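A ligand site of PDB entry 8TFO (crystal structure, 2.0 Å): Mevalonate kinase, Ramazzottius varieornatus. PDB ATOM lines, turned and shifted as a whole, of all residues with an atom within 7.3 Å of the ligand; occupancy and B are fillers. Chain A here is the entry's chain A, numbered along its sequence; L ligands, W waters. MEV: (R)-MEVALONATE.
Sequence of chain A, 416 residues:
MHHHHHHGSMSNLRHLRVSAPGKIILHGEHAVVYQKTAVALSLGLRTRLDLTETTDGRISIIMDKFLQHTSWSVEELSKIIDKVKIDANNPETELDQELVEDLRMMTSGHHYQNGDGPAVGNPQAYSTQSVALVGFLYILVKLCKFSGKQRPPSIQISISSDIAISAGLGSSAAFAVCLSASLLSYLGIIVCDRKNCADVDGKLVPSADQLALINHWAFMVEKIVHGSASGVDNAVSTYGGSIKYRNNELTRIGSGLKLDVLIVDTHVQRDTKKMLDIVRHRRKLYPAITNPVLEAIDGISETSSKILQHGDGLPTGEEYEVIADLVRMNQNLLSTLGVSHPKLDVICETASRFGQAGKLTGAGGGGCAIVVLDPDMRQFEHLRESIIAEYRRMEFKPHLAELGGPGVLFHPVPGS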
ATOM      1  N   LYS A  23      19.848   8.970   1.375  1.00  0.00           N
ATOM      2  CA  LYS A  23      20.357   8.980   2.745  1.00  0.00           C
ATOM      3  C   LYS A  23      21.405   7.872   2.939  1.00  0.00           C
ATOM      4  O   LYS A  23      21.447   6.885   2.201  1.00  0.00           O
ATOM      5  CB  LYS A  23      19.216   8.858   3.766  1.00  0.00           C
ATOM      6  CG  LYS A  23      18.396   7.577   3.654  1.00  0.00           C
ATOM      7  CD  LYS A  23      19.009   6.358   4.356  1.00  0.00           C
ATOM      8  CE  LYS A  23      18.722   5.078   3.610  1.00  0.00           C
ATOM      9  NZ  LYS A  23      19.069   3.866   4.376  1.00  0.00           N
ATOM     10  N   ILE A  25      22.989   5.782   6.575  1.00  0.00           N
ATOM     11  CA  ILE A  25      22.941   5.595   8.005  1.00  0.00           C
ATOM     12  C   ILE A  25      24.387   5.480   8.493  1.00  0.00           C
ATOM     13  O   ILE A  25      25.108   4.582   8.068  1.00  0.00           O
ATOM     14  CB  ILE A  25      22.070   4.375   8.351  1.00  0.00           C
ATOM     15  CG1 ILE A  25      20.638   4.575   7.848  1.00  0.00           C
ATOM     16  CG2 ILE A  25      22.125   4.087   9.849  1.00  0.00           C
ATOM     17  CD1 ILE A  25      19.745   3.364   8.045  1.00  0.00           C
ATOM     18  N   GLY A  28      23.574   2.451  13.453  1.00  0.00           N
ATOM     19  CA  GLY A  28      22.366   1.992  14.108  1.00  0.00           C
ATOM     20  C   GLY A  28      21.399   1.293  13.159  1.00  0.00           C
ATOM     21  O   GLY A  28      20.320   0.890  13.593  1.00  0.00           O
ATOM     22  N   GLU A  29      21.782   1.081  11.886  1.00  0.00           N
ATOM     23  CA  GLU A  29      20.965   0.221  11.035  1.00  0.00           C
ATOM     24  C   GLU A  29      20.802  -1.134  11.722  1.00  0.00           C
ATOM     25  O   GLU A  29      21.685  -1.582  12.456  1.00  0.00           O
ATOM     26  CB  GLU A  29      21.517   0.041   9.623  1.00  0.00           C
ATOM     27  CG  GLU A  29      22.972  -0.401   9.555  1.00  0.00           C
ATOM     28  CD  GLU A  29      23.940   0.765   9.495  1.00  0.00           C
ATOM     29  OE1 GLU A  29      24.076   1.310   8.409  1.00  0.00           O
ATOM     30  OE2 GLU A  29      24.535   1.141  10.556  1.00  0.00           O
ATOM     31  N   HIS A  30      19.637  -1.755  11.487  1.00  0.00           N
ATOM     32  CA  HIS A  30      19.207  -3.045  12.022  1.00  0.00           C
ATOM     33  C   HIS A  30      18.855  -2.963  13.504  1.00  0.00           C
ATOM     34  O   HIS A  30      17.803  -3.448  13.923  1.00  0.00           O
ATOM     35  CB  HIS A  30      20.187  -4.153  11.676  1.00  0.00           C
ATOM     36  CG  HIS A  30      20.107  -4.640  10.279  1.00  0.00           C
ATOM     37  ND1 HIS A  30      19.056  -5.412   9.827  1.00  0.00           N
ATOM     38  CD2 HIS A  30      20.974  -4.542   9.251  1.00  0.00           C
ATOM     39  CE1 HIS A  30      19.268  -5.723   8.546  1.00  0.00           C
ATOM     40  NE2 HIS A  30      20.431  -5.193   8.166  1.00  0.00           N
ATOM     41  N   ALA A  31      19.734  -2.387  14.327  1.00  0.00           N
ATOM     42  CA  ALA A  31      19.421  -2.160  15.736  1.00  0.00           C
ATOM     43  C   ALA A  31      18.181  -1.271  15.869  1.00  0.00           C
ATOM     44  O   ALA A  31      17.364  -1.444  16.797  1.00  0.00           O
ATOM     45  CB  ALA A  31      20.604  -1.560  16.443  1.00  0.00           C
ATOM     46  N   VAL A  32      18.090  -0.296  14.963  1.00  0.00           N
ATOM     47  CA  VAL A  32      17.045   0.725  15.032  1.00  0.00           C
ATOM     48  C   VAL A  32      15.669   0.085  14.902  1.00  0.00           C
ATOM     49  O   VAL A  32      14.702   0.634  15.431  1.00  0.00           O
ATOM     50  CB  VAL A  32      17.262   1.834  13.980  1.00  0.00           C
ATOM     51  CG1 VAL A  32      17.119   1.326  12.555  1.00  0.00           C
ATOM     52  CG2 VAL A  32      16.363   3.032  14.210  1.00  0.00           C
ATOM     53  N   VAL A  33      15.602  -1.062  14.227  1.00  0.00           N
ATOM     54  CA  VAL A  33      14.374  -1.832  14.092  1.00  0.00           C
ATOM     55  C   VAL A  33      13.868  -2.298  15.470  1.00  0.00           C
ATOM     56  O   VAL A  33      12.686  -2.514  15.633  1.00  0.00           O
ATOM     57  CB  VAL A  33      14.593  -3.046  13.167  1.00  0.00           C
ATOM     58  CG1 VAL A  33      13.364  -3.929  13.096  1.00  0.00           C
ATOM     59  CG2 VAL A  33      15.033  -2.655  11.757  1.00  0.00           C
ATOM     60  N   ALA A  38      19.716   5.392  16.051  1.00  0.00           N
ATOM     61  CA  ALA A  38      20.449   5.496  14.808  1.00  0.00           C
ATOM     62  C   ALA A  38      20.817   6.955  14.550  1.00  0.00           C
ATOM     63  O   ALA A  38      20.194   7.868  15.076  1.00  0.00           O
ATOM     64  CB  ALA A  38      19.660   4.918  13.656  1.00  0.00           C
ATOM     65  N   GLY A 168      20.768   0.864  -1.635  1.00  0.00           N
ATOM     66  CA  GLY A 168      20.553   1.064  -0.201  1.00  0.00           C
ATOM     67  C   GLY A 168      20.866   2.489   0.239  1.00  0.00           C
ATOM     68  O   GLY A 168      21.353   2.718   1.358  1.00  0.00           O
ATOM     69  N   LEU A 169      20.531   3.451  -0.633  1.00  0.00           N
ATOM     70  CA  LEU A 169      20.745   4.876  -0.358  1.00  0.00           C
ATOM     71  C   LEU A 169      19.406   5.624  -0.257  1.00  0.00           C
ATOM     72  O   LEU A 169      19.377   6.842  -0.410  1.00  0.00           O
ATOM     73  CB  LEU A 169      21.606   5.455  -1.491  1.00  0.00           C
ATOM     74  CG  LEU A 169      23.017   4.874  -1.661  1.00  0.00           C
ATOM     75  CD1 LEU A 169      23.736   5.549  -2.819  1.00  0.00           C
ATOM     76  CD2 LEU A 169      23.849   5.003  -0.391  1.00  0.00           C
ATOM     77  N   GLY A 170      18.309   4.919   0.022  1.00  0.00           N
ATOM     78  CA  GLY A 170      17.052   5.571   0.374  1.00  0.00           C
ATOM     79  C   GLY A 170      16.128   5.825  -0.827  1.00  0.00           C
ATOM     80  O   GLY A 170      15.240   6.663  -0.741  1.00  0.00           O
ATOM     81  N   PHE A 219       6.004   6.974   5.928  1.00  0.00           N
ATOM     82  CA  PHE A 219       6.305   5.794   6.732  1.00  0.00           C
ATOM     83  C   PHE A 219       5.385   4.640   6.327  1.00  0.00           C
ATOM     84  O   PHE A 219       5.833   3.504   6.204  1.00  0.00           O
ATOM     85  CB  PHE A 219       6.187   6.109   8.230  1.00  0.00           C
ATOM     86  CG  PHE A 219       6.785   5.112   9.195  1.00  0.00           C
ATOM     87  CD1 PHE A 219       7.552   4.044   8.762  1.00  0.00           C
ATOM     88  CD2 PHE A 219       6.593   5.263  10.578  1.00  0.00           C
ATOM     89  CE1 PHE A 219       8.107   3.147   9.661  1.00  0.00           C
ATOM     90  CE2 PHE A 219       7.147   4.352  11.482  1.00  0.00           C
ATOM     91  CZ  PHE A 219       7.902   3.296  11.017  1.00  0.00           C
ATOM     92  N   GLU A 222       6.616   3.025   3.355  1.00  0.00           N
ATOM     93  CA  GLU A 222       7.829   2.271   3.640  1.00  0.00           C
ATOM     94  C   GLU A 222       7.470   0.939   4.298  1.00  0.00           C
ATOM     95  O   GLU A 222       8.106  -0.085   3.990  1.00  0.00           O
ATOM     96  CB  GLU A 222       8.775   3.116   4.490  1.00  0.00           C
ATOM     97  CG  GLU A 222       9.591   4.100   3.665  1.00  0.00           C
ATOM     98  CD  GLU A 222      10.754   3.416   2.957  1.00  0.00           C
ATOM     99  OE1 GLU A 222      11.735   3.110   3.642  1.00  0.00           O
ATOM    100  OE2 GLU A 222      10.619   3.109   1.779  1.00  0.00           O
ATOM    101  N   HIS A 226       8.726  -2.742   3.233  1.00  0.00           N
ATOM    102  CA  HIS A 226       9.335  -3.623   4.228  1.00  0.00           C
ATOM    103  C   HIS A 226       8.619  -3.435   5.572  1.00  0.00           C
ATOM    104  O   HIS A 226       8.745  -2.389   6.229  1.00  0.00           O
ATOM    105  CB  HIS A 226      10.848  -3.382   4.334  1.00  0.00           C
ATOM    106  CG  HIS A 226      11.380  -2.219   3.546  1.00  0.00           C
ATOM    107  ND1 HIS A 226      11.146  -0.887   3.850  1.00  0.00           N
ATOM    108  CD2 HIS A 226      12.159  -2.203   2.445  1.00  0.00           C
ATOM    109  CE1 HIS A 226      11.771  -0.108   2.970  1.00  0.00           C
ATOM    110  NE2 HIS A 226      12.400  -0.885   2.110  1.00  0.00           N
ATOM    111  N   SER A 228       8.679  -4.186   8.705  1.00  0.00           N
ATOM    112  CA  SER A 228       9.219  -3.772   9.992  1.00  0.00           C
ATOM    113  C   SER A 228      10.229  -2.618   9.839  1.00  0.00           C
ATOM    114  O   SER A 228      11.115  -2.455  10.685  1.00  0.00           O
ATOM    115  CB  SER A 228       9.785  -4.959  10.754  1.00  0.00           C
ATOM    116  OG  SER A 228      10.760  -5.627   9.978  1.00  0.00           O
ATOM    117  N   ALA A 229      10.073  -1.760   8.827  1.00  0.00           N
ATOM    118  CA  ALA A 229      10.880  -0.549   8.722  1.00  0.00           C
ATOM    119  C   ALA A 229      10.825   0.223  10.037  1.00  0.00           C
ATOM    120  O   ALA A 229       9.772   0.311  10.649  1.00  0.00           O
ATOM    121  CB  ALA A 229      10.382   0.323   7.592  1.00  0.00           C
ATOM    122  N   SER A 230      11.961   0.774  10.447  1.00  0.00           N
ATOM    123  CA  SER A 230      12.083   1.569  11.664  1.00  0.00           C
ATOM    124  C   SER A 230      11.471   2.951  11.482  1.00  0.00           C
ATOM    125  O   SER A 230      11.039   3.576  12.454  1.00  0.00           O
ATOM    126  CB  SER A 230      13.535   1.699  12.062  1.00  0.00           C
ATOM    127  OG  SER A 230      14.276   2.492  11.131  1.00  0.00           O
ATOM    128  N   GLY A 231      11.470   3.449  10.245  1.00  0.00           N
ATOM    129  CA  GLY A 231      11.041   4.821   9.979  1.00  0.00           C
ATOM    130  C   GLY A 231      12.208   5.821   9.947  1.00  0.00           C
ATOM    131  O   GLY A 231      12.001   7.017   9.686  1.00  0.00           O
ATOM    132  N   VAL A 232      13.438   5.344  10.190  1.00  0.00           N
ATOM    133  CA  VAL A 232      14.586   6.236  10.168  1.00  0.00           C
ATOM    134  C   VAL A 232      14.767   6.796   8.752  1.00  0.00           C
ATOM    135  O   VAL A 232      15.149   7.948   8.604  1.00  0.00           O
ATOM    136  CB  VAL A 232      15.877   5.559  10.659  1.00  0.00           C
ATOM    137  CG1 VAL A 232      16.399   4.482   9.700  1.00  0.00           C
ATOM    138  CG2 VAL A 232      16.969   6.587  10.906  1.00  0.00           C
ATOM    139  N   ASP A 233      14.547   5.955   7.730  1.00  0.00           N
ATOM    140  CA  ASP A 233      14.838   6.310   6.343  1.00  0.00           C
ATOM    141  C   ASP A 233      13.911   7.429   5.840  1.00  0.00           C
ATOM    142  O   ASP A 233      14.382   8.426   5.273  1.00  0.00           O
ATOM    143  CB  ASP A 233      14.768   5.070   5.428  1.00  0.00           C
ATOM    144  CG  ASP A 233      15.943   4.130   5.586  1.00  0.00           C
ATOM    145  OD1 ASP A 233      16.950   4.498   6.265  1.00  0.00           O
ATOM    146  OD2 ASP A 233      15.890   3.026   4.991  1.00  0.00           O
ATOM    147  N   ASN A 234      12.605   7.263   6.060  1.00  0.00           N
ATOM    148  CA  ASN A 234      11.643   8.261   5.657  1.00  0.00           C
ATOM    149  C   ASN A 234      11.856   9.515   6.486  1.00  0.00           C
ATOM    150  O   ASN A 234      11.670  10.623   5.960  1.00  0.00           O
ATOM    151  CB  ASN A 234      10.185   7.784   5.719  1.00  0.00           C
ATOM    152  CG  ASN A 234       9.845   6.989   6.957  1.00  0.00           C
ATOM    153  OD1 ASN A 234       9.999   5.763   6.957  1.00  0.00           O
ATOM    154  ND2 ASN A 234       9.347   7.665   7.975  1.00  0.00           N
ATOM    155  N   TYR A 245      17.823   9.313  15.772  1.00  0.00           N
ATOM    156  CA  TYR A 245      16.487   8.759  15.660  1.00  0.00           C
ATOM    157  C   TYR A 245      16.374   7.536  16.533  1.00  0.00           C
ATOM    158  O   TYR A 245      17.268   6.704  16.551  1.00  0.00           O
ATOM    159  CB  TYR A 245      16.206   8.372  14.215  1.00  0.00           C
ATOM    160  CG  TYR A 245      14.843   7.762  13.920  1.00  0.00           C
ATOM    161  CD1 TYR A 245      14.616   6.404  14.059  1.00  0.00           C
ATOM    162  CD2 TYR A 245      13.796   8.537  13.465  1.00  0.00           C
ATOM    163  CE1 TYR A 245      13.388   5.830  13.780  1.00  0.00           C
ATOM    164  CE2 TYR A 245      12.552   7.979  13.163  1.00  0.00           C
ATOM    165  CZ  TYR A 245      12.362   6.626  13.303  1.00  0.00           C
ATOM    166  OH  TYR A 245      11.143   6.099  12.988  1.00  0.00           O
ATOM    167  N   THR A 272      15.861  -6.035   1.056  1.00  0.00           N
ATOM    168  CA  THR A 272      15.961  -5.568   2.423  1.00  0.00           C
ATOM    169  C   THR A 272      15.265  -6.544   3.372  1.00  0.00           C
ATOM    170  O   THR A 272      15.708  -6.775   4.500  1.00  0.00           O
ATOM    171  CB  THR A 272      15.418  -4.143   2.582  1.00  0.00           C
ATOM    172  OG1 THR A 272      16.378  -3.316   1.930  1.00  0.00           O
ATOM    173  CG2 THR A 272      15.257  -3.689   4.022  1.00  0.00           C
ATOM    174  N   MET A 275      17.346  -9.355   4.662  1.00  0.00           N
ATOM    175  CA  MET A 275      18.355  -8.964   5.641  1.00  0.00           C
ATOM    176  C   MET A 275      17.687  -8.796   7.001  1.00  0.00           C
ATOM    177  O   MET A 275      18.182  -9.314   7.984  1.00  0.00           O
ATOM    178  CB  MET A 275      19.081  -7.671   5.245  1.00  0.00           C
ATOM    179  CG  MET A 275      19.688  -7.737   3.868  1.00  0.00           C
ATOM    180  SD  MET A 275      20.670  -9.212   3.570  1.00  0.00           S
ATOM    181  CE  MET A 275      21.908  -9.018   4.851  1.00  0.00           C
ATOM    182  N   LEU A 276      16.533  -8.144   7.029  1.00  0.00           N
ATOM    183  CA  LEU A 276      15.777  -8.015   8.266  1.00  0.00           C
ATOM    184  C   LEU A 276      15.459  -9.386   8.864  1.00  0.00           C
ATOM    185  O   LEU A 276      15.469  -9.544  10.067  1.00  0.00           O
ATOM    186  CB  LEU A 276      14.492  -7.232   7.988  1.00  0.00           C
ATOM    187  CG  LEU A 276      14.672  -5.770   7.563  1.00  0.00           C
ATOM    188  CD1 LEU A 276      13.337  -5.162   7.103  1.00  0.00           C
ATOM    189  CD2 LEU A 276      15.272  -4.938   8.681  1.00  0.00           C
ATOM    190  N   THR A 361      26.182   0.464   4.989  1.00  0.00           N
ATOM    191  CA  THR A 361      25.105   1.332   5.444  1.00  0.00           C
ATOM    192  C   THR A 361      23.780   0.714   4.985  1.00  0.00           C
ATOM    193  O   THR A 361      23.656   0.242   3.873  1.00  0.00           O
ATOM    194  CB  THR A 361      25.307   2.774   4.944  1.00  0.00           C
ATOM    195  OG1 THR A 361      24.305   3.609   5.510  1.00  0.00           O
ATOM    196  CG2 THR A 361      25.280   2.894   3.442  1.00  0.00           C
ATOM    197  N   GLY A 362      22.782   0.705   5.860  1.00  0.00           N
ATOM    198  CA  GLY A 362      21.471   0.184   5.506  1.00  0.00           C
ATOM    199  C   GLY A 362      21.367  -1.310   5.768  1.00  0.00           C
ATOM    200  O   GLY A 362      21.883  -1.807   6.752  1.00  0.00           O
ATOM    201  N   ALA A 363      20.733  -2.026   4.844  1.00  0.00           N
ATOM    202  CA  ALA A 363      20.306  -3.400   5.036  1.00  0.00           C
ATOM    203  C   ALA A 363      21.493  -4.364   5.024  1.00  0.00           C
ATOM    204  O   ALA A 363      21.435  -5.402   5.667  1.00  0.00           O
ATOM    205  CB  ALA A 363      19.316  -3.740   3.953  1.00  0.00           C
ATOM    206  N   GLY A 364      22.529  -4.015   4.263  1.00  0.00           N
ATOM    207  CA  GLY A 364      23.679  -4.872   4.061  1.00  0.00           C
ATOM    208  C   GLY A 364      23.403  -5.993   3.065  1.00  0.00           C
ATOM    209  O   GLY A 364      22.430  -5.932   2.329  1.00  0.00           O
HETATM  210  C8  MEV L   1      17.252   0.262   6.174  1.00  0.00           C
HETATM  211  O8  MEV L   1      18.002   1.142   5.362  1.00  0.00           O
HETATM  212  C2  MEV L   1      17.807   0.268   7.563  1.00  0.00           C
HETATM  213  C3  MEV L   1      17.388  -0.908   8.458  1.00  0.00           C
HETATM  214  O7  MEV L   1      17.783  -0.576   9.810  1.00  0.00           O
HETATM  215  C4  MEV L   1      15.867  -1.113   8.369  1.00  0.00           C
HETATM  216  C5  MEV L   1      15.086   0.080   8.875  1.00  0.00           C
HETATM  217  O3  MEV L   1      14.019   0.330   8.315  1.00  0.00           O
HETATM  218  O4  MEV L   1      15.540   0.735   9.832  1.00  0.00           O
HETATM  219  C6  MEV L   1      18.114  -2.188   8.100  1.00  0.00           C
HETATM  220  O   HOH W   1      13.375   3.099   8.120  1.00  0.00           O
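The backbone NH of Ser 230 lies within hydrogen-bond range of an oxygen (O3) of the ligand (3.0 Å).
An oxygen (O4) of the ligand lies within hydrogen-bond range of the side-chain hydroxyl (OG) of Ser 230, 2.5 Å away.
O7 of the ligand is in hydrogen-bond range of N of His 30, at 2.8 Å.
An oxygen (O8) of the ligand lies within hydrogen-bond range of the side-chain carboxylate of Asp 233 (2.9 Å).
The side-chain amino group (NZ) of Lys 23 is in hydrogen-bond range of an oxygen (O8) of the ligand, 3.1 Å away.
OG of Ser 230 sits at hydrogen-bond distance from N of Val 232 (3.1 Å).
OH of Tyr 245 lies within hydrogen-bond range of O of Ser 230.
The backbone carbonyl oxygen (O) of Ala 363 sits at hydrogen-bond distance from a ring nitrogen (NE2) of His 30 (2.7 Å).
The side-chain carboxylate of Asp 233 is in salt-bridge range of the side-chain amino group of Lys 23 (2.9 Å).
N of Lys 23 sits at hydrogen-bond distance from O of Leu 169.
The side-chain carboxylate (OE1) of Glu 29 sits at hydrogen-bond distance from the backbone NH (N) of Gly 362, at 2.9 Å.
The side-chain hydroxyl of Thr 361 lies within hydrogen-bond range of the backbone NH of Ile 25, 2.8 Å away.
Merely in contact with the ligand: Ile 25, Glu 29, Val 32, Val 33, Ala 229, Val 232, Leu 276, Gly 362 and Ala 363.
13 residues have an atom within 4 Å of the ligand: Lys 23, Ile 25, Glu 29, His 30, Val 32, Val 33, Ala 229, Ser 230, Val 232, Asp 233, Leu 276, Gly 362 and Ala 363.
The nearest printed residue that does not touch the ligand is Gly 231 (4.5 Å).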
